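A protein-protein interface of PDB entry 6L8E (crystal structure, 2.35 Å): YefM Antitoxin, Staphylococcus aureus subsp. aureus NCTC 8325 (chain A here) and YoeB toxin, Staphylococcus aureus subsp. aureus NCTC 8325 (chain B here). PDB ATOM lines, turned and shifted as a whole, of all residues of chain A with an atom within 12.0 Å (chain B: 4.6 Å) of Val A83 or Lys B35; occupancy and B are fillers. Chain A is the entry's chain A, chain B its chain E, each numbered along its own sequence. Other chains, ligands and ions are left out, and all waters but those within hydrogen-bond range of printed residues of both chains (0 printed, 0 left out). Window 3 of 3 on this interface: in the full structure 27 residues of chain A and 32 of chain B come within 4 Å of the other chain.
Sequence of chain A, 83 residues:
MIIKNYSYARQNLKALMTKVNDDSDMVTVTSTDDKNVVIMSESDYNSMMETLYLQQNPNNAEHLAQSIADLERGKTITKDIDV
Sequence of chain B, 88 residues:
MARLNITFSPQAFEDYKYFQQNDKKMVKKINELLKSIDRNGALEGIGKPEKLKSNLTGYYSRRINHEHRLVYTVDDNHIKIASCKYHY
N of Val A83 sits at hydrogen-bond distance from O of Ala B2 (2.5 Å). The chain-end carboxylate (OXT) of Val A83 is in salt-bridge range of the side-chain amino group (NZ) of Lys B35, 3.7 Å away. N of Leu B4 is in hydrogen-bond range of O of Ile A81 (2.8 Å).
Among the printed residues, merely in contact across the chains: Asp A82 with Ala B2 (3.2 Å), Asp A80 with Leu B4 (3.2 Å), Val A83 with Asn B31 (3.3 Å), Ile A81 with Asn B31 (3.5 Å), Ile A81 with Ala B2 (3.6 Å), Lys A79 with Leu B4 (3.7 Å), Asp A82 with Asn B31 (3.9 Å), Ile A81 with Leu B34 (3.95 Å) and Val A83 with Leu B4 (3.95 Å).
Of the printed residues of chain A, Lys B35 touches Val A83. Ala B2 touches just these residues of chain A: Ile A81, Asp A82 and Val A83. Of chain A, only Lys A79, Asp A80, Ile A81 and Val A83 come within 4 Å of Leu B4. Of chain A, only Ile A81, Asp A82 and Val A83 come within 4 Å of Asn B31. Leu B34 touches just one residue of chain A: Ile A81. No residue of chain A comes within 4 Å of Ser B36. Ile B37 touches none of the printed residues of chain A. No residue of chain A comes within 4 Å of Asp B38. Printed residues of chain B within 4 Å of Asp A80: Leu B4. Of the printed residues of chain B, Lys A79 touches Leu B4 (3.7 Å). Printed residues of chain B within 4 Å of Asp A82: Ala B2 and Asn B31. Printed residues of chain B within 4 Å of Ile A81: Ala B2, Leu B4, Asn B31 and Leu B34. Glu B32 touches none of the printed residues of chain A. Arg B39 touches none of the printed residues of chain A. The nearest residue of chain B that does not touch Val A83 is Leu B34 (4.5 Å). The nearest residue of chain A that does not touch Lys B35 is Ile A81 (7.5 Å). The nearest printed residue of chain B that does not touch Asp A80 is Ala B2 (7.3 Å).
Of the 5 printed residues of chain A, 5 touch a printed residue of chain B. Hydrophobic or aromatic side chains of chain A within 4 Å of the printed part of chain B: Ile A81 and Val A83. Along chain A the printed residues that touch a printed residue of chain B span positions 79 to 83. Printed residues of chain B that touch a printed residue of chain A: Ala B2, Leu B4, Asn B31, Leu B34 and Lys B35. Hydrophobic or aromatic side chains of chain B within 4 Å of the printed part of chain A: Leu B4 and Leu B34. Among the printed residues, no Asp or Glu carboxylate lies within 4 Å of a Lys or Arg side-chain nitrogen of the other chain.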
ATOM      1  N   LYS A  79      14.955  25.898 -33.013  1.00  0.00           N
ATOM      2  CA  LYS A  79      16.083  25.282 -32.341  1.00  0.00           C
ATOM      3  C   LYS A  79      15.918  23.771 -32.370  1.00  0.00           C
ATOM      4  O   LYS A  79      14.800  23.252 -32.317  1.00  0.00           O
ATOM      5  CB  LYS A  79      16.216  25.757 -30.891  1.00  0.00           C
ATOM      6  CG  LYS A  79      16.767  27.159 -30.756  1.00  0.00           C
ATOM      7  CD  LYS A  79      17.272  27.419 -29.349  1.00  0.00           C
ATOM      8  CE  LYS A  79      18.334  26.396 -28.950  1.00  0.00           C
ATOM      9  NZ  LYS A  79      19.550  26.498 -29.813  1.00  0.00           N
ATOM     10  N   ASP A  80      17.047  23.076 -32.477  1.00  0.00           N
ATOM     11  CA  ASP A  80      17.118  21.636 -32.277  1.00  0.00           C
ATOM     12  C   ASP A  80      17.772  21.380 -30.928  1.00  0.00           C
ATOM     13  O   ASP A  80      18.880  21.860 -30.672  1.00  0.00           O
ATOM     14  CB  ASP A  80      17.901  20.958 -33.398  1.00  0.00           C
ATOM     15  CG  ASP A  80      17.183  21.021 -34.724  1.00  0.00           C
ATOM     16  OD1 ASP A  80      15.933  20.993 -34.727  1.00  0.00           O
ATOM     17  OD2 ASP A  80      17.861  21.107 -35.765  1.00  0.00           O
ATOM     18  N   ILE A  81      17.081  20.640 -30.067  1.00  0.00           N
ATOM     19  CA  ILE A  81      17.478  20.484 -28.675  1.00  0.00           C
ATOM     20  C   ILE A  81      17.594  19.001 -28.363  1.00  0.00           C
ATOM     21  O   ILE A  81      16.625  18.250 -28.527  1.00  0.00           O
ATOM     22  CB  ILE A  81      16.486  21.166 -27.724  1.00  0.00           C
ATOM     23  CG1 ILE A  81      16.571  22.683 -27.895  1.00  0.00           C
ATOM     24  CG2 ILE A  81      16.764  20.777 -26.282  1.00  0.00           C
ATOM     25  CD1 ILE A  81      15.492  23.447 -27.174  1.00  0.00           C
ATOM     26  N   ASP A  82      18.780  18.582 -27.921  1.00  0.00           N
ATOM     27  CA  ASP A  82      18.993  17.213 -27.477  1.00  0.00           C
ATOM     28  C   ASP A  82      18.403  17.043 -26.086  1.00  0.00           C
ATOM     29  O   ASP A  82      18.669  17.842 -25.184  1.00  0.00           O
ATOM     30  CB  ASP A  82      20.481  16.872 -27.494  1.00  0.00           C
ATOM     31  CG  ASP A  82      21.020  16.738 -28.900  1.00  0.00           C
ATOM     32  OD1 ASP A  82      20.441  15.953 -29.684  1.00  0.00           O
ATOM     33  OD2 ASP A  82      21.999  17.436 -29.234  1.00  0.00           O
ATOM     34  N   VAL A  83      17.597  16.004 -25.918  1.00  0.00           N
ATOM     35  CA  VAL A  83      16.661  15.954 -24.809  1.00  0.00           C
ATOM     36  C   VAL A  83      16.668  14.591 -24.119  1.00  0.00           C
ATOM     37  O   VAL A  83      16.858  13.550 -24.756  1.00  0.00           O
ATOM     38  CB  VAL A  83      15.249  16.333 -25.319  1.00  0.00           C
ATOM     39  CG1 VAL A  83      14.254  15.213 -25.095  1.00  0.00           C
ATOM     40  CG2 VAL A  83      14.778  17.630 -24.685  1.00  0.00           C
ATOM     41  OXT VAL A  83      16.493  14.505 -22.902  1.00  0.00           O
ATOM     42  N   ALA B   2      15.097  11.987 -29.069  1.00  0.00           N
ATOM     43  CA  ALA B   2      16.196  12.534 -28.283  1.00  0.00           C
ATOM     44  C   ALA B   2      16.601  13.926 -28.759  1.00  0.00           C
ATOM     45  O   ALA B   2      17.015  14.762 -27.960  1.00  0.00           O
ATOM     46  CB  ALA B   2      17.391  11.601 -28.327  1.00  0.00           C
ATOM     47  N   LEU B   4      14.952  17.088 -30.505  1.00  0.00           N
ATOM     48  CA  LEU B   4      13.642  17.650 -30.788  1.00  0.00           C
ATOM     49  C   LEU B   4      13.763  18.930 -31.604  1.00  0.00           C
ATOM     50  O   LEU B   4      14.721  19.692 -31.456  1.00  0.00           O
ATOM     51  CB  LEU B   4      12.879  17.950 -29.494  1.00  0.00           C
ATOM     52  CG  LEU B   4      12.572  16.760 -28.584  1.00  0.00           C
ATOM     53  CD1 LEU B   4      11.728  17.201 -27.399  1.00  0.00           C
ATOM     54  CD2 LEU B   4      11.880  15.654 -29.363  1.00  0.00           C
ATOM     55  N   ASN B  31      14.604  21.687 -20.727  1.00  0.00           N
ATOM     56  CA  ASN B  31      14.716  20.551 -21.636  1.00  0.00           C
ATOM     57  C   ASN B  31      13.965  19.341 -21.101  1.00  0.00           C
ATOM     58  O   ASN B  31      13.369  18.582 -21.873  1.00  0.00           O
ATOM     59  CB  ASN B  31      16.188  20.217 -21.868  1.00  0.00           C
ATOM     60  CG  ASN B  31      16.893  21.271 -22.693  1.00  0.00           C
ATOM     61  OD1 ASN B  31      16.318  22.315 -23.004  1.00  0.00           O
ATOM     62  ND2 ASN B  31      18.143  21.007 -23.050  1.00  0.00           N
ATOM     63  N   GLU B  32      13.976  19.149 -19.782  1.00  0.00           N
ATOM     64  CA  GLU B  32      13.201  18.062 -19.193  1.00  0.00           C
ATOM     65  C   GLU B  32      11.705  18.291 -19.367  1.00  0.00           C
ATOM     66  O   GLU B  32      10.952  17.338 -19.599  1.00  0.00           O
ATOM     67  CB  GLU B  32      13.553  17.912 -17.715  1.00  0.00           C
ATOM     68  CG  GLU B  32      14.957  17.385 -17.460  1.00  0.00           C
ATOM     69  CD  GLU B  32      15.396  17.616 -16.028  1.00  0.00           C
ATOM     70  OE1 GLU B  32      14.656  18.313 -15.304  1.00  0.00           O
ATOM     71  OE2 GLU B  32      16.470  17.112 -15.629  1.00  0.00           O
ATOM     72  N   LEU B  33      11.257  19.545 -19.244  1.00  0.00           N
ATOM     73  CA  LEU B  33       9.852  19.862 -19.494  1.00  0.00           C
ATOM     74  C   LEU B  33       9.481  19.592 -20.946  1.00  0.00           C
ATOM     75  O   LEU B  33       8.411  19.039 -21.230  1.00  0.00           O
ATOM     76  CB  LEU B  33       9.564  21.320 -19.137  1.00  0.00           C
ATOM     77  CG  LEU B  33       9.761  21.771 -17.691  1.00  0.00           C
ATOM     78  CD1 LEU B  33       9.549  23.271 -17.589  1.00  0.00           C
ATOM     79  CD2 LEU B  33       8.812  21.028 -16.764  1.00  0.00           C
ATOM     80  N   LEU B  34      10.356  19.982 -21.878  1.00  0.00           N
ATOM     81  CA  LEU B  34      10.117  19.725 -23.294  1.00  0.00           C
ATOM     82  C   LEU B  34      10.014  18.230 -23.572  1.00  0.00           C
ATOM     83  O   LEU B  34       9.130  17.790 -24.317  1.00  0.00           O
ATOM     84  CB  LEU B  34      11.223  20.364 -24.139  1.00  0.00           C
ATOM     85  CG  LEU B  34      11.222  21.892 -24.152  1.00  0.00           C
ATOM     86  CD1 LEU B  34      12.440  22.453 -24.869  1.00  0.00           C
ATOM     87  CD2 LEU B  34       9.941  22.392 -24.797  1.00  0.00           C
ATOM     88  N   LYS B  35      10.901  17.432 -22.970  1.00  0.00           N
ATOM     89  CA  LYS B  35      10.813  15.984 -23.134  1.00  0.00           C
ATOM     90  C   LYS B  35       9.475  15.459 -22.630  1.00  0.00           C
ATOM     91  O   LYS B  35       8.841  14.623 -23.283  1.00  0.00           O
ATOM     92  CB  LYS B  35      11.963  15.285 -22.411  1.00  0.00           C
ATOM     93  CG  LYS B  35      12.036  13.792 -22.713  1.00  0.00           C
ATOM     94  CD  LYS B  35      12.512  12.983 -21.518  1.00  0.00           C
ATOM     95  CE  LYS B  35      14.029  12.957 -21.415  1.00  0.00           C
ATOM     96  NZ  LYS B  35      14.582  11.581 -21.589  1.00  0.00           N
ATOM     97  N   SER B  36       9.024  15.950 -21.474  1.00  0.00           N
ATOM     98  CA  SER B  36       7.744  15.510 -20.931  1.00  0.00           C
ATOM     99  C   SER B  36       6.591  15.896 -21.850  1.00  0.00           C
ATOM    100  O   SER B  36       5.682  15.092 -22.091  1.00  0.00           O
ATOM    101  CB  SER B  36       7.539  16.096 -19.537  1.00  0.00           C
ATOM    102  OG  SER B  36       6.302  15.686 -18.984  1.00  0.00           O
ATOM    103  N   ILE B  37       6.604  17.133 -22.358  1.00  0.00           N
ATOM    104  CA  ILE B  37       5.570  17.577 -23.290  1.00  0.00           C
ATOM    105  C   ILE B  37       5.552  16.693 -24.528  1.00  0.00           C
ATOM    106  O   ILE B  37       4.487  16.273 -24.994  1.00  0.00           O
ATOM    107  CB  ILE B  37       5.783  19.057 -23.658  1.00  0.00           C
ATOM    108  CG1 ILE B  37       5.569  19.949 -22.437  1.00  0.00           C
ATOM    109  CG2 ILE B  37       4.843  19.475 -24.780  1.00  0.00           C
ATOM    110  CD1 ILE B  37       6.167  21.321 -22.589  1.00  0.00           C
ATOM    111  N   ASP B  38       6.732  16.385 -25.072  1.00  0.00           N
ATOM    112  CA  ASP B  38       6.804  15.558 -26.272  1.00  0.00           C
ATOM    113  C   ASP B  38       6.316  14.142 -26.001  1.00  0.00           C
ATOM    114  O   ASP B  38       5.679  13.521 -26.860  1.00  0.00           O
ATOM    115  CB  ASP B  38       8.235  15.538 -26.808  1.00  0.00           C
ATOM    116  CG  ASP B  38       8.385  14.673 -28.043  1.00  0.00           C
ATOM    117  OD1 ASP B  38       7.800  15.027 -29.089  1.00  0.00           O
ATOM    118  OD2 ASP B  38       9.089  13.645 -27.973  1.00  0.00           O
ATOM    119  N   ARG B  39       6.594  13.616 -24.810  1.00  0.00           N
ATOM    120  CA  ARG B  39       6.244  12.229 -24.525  1.00  0.00           C
ATOM    121  C   ARG B  39       4.776  12.085 -24.138  1.00  0.00           C
ATOM    122  O   ARG B  39       4.112  11.138 -24.571  1.00  0.00           O
ATOM    123  CB  ARG B  39       7.151  11.679 -23.424  1.00  0.00           C
ATOM    124  CG  ARG B  39       7.176  10.162 -23.349  1.00  0.00           C
ATOM    125  CD  ARG B  39       8.218   9.669 -22.354  1.00  0.00           C
ATOM    126  NE  ARG B  39       8.049   8.252 -22.047  1.00  0.00           N
ATOM    127  CZ  ARG B  39       7.192   7.786 -21.142  1.00  0.00           C
ATOM    128  NH1 ARG B  39       6.428   8.628 -20.460  1.00  0.00           N
ATOM    129  NH2 ARG B  39       7.095   6.481 -20.922  1.00  0.00           N
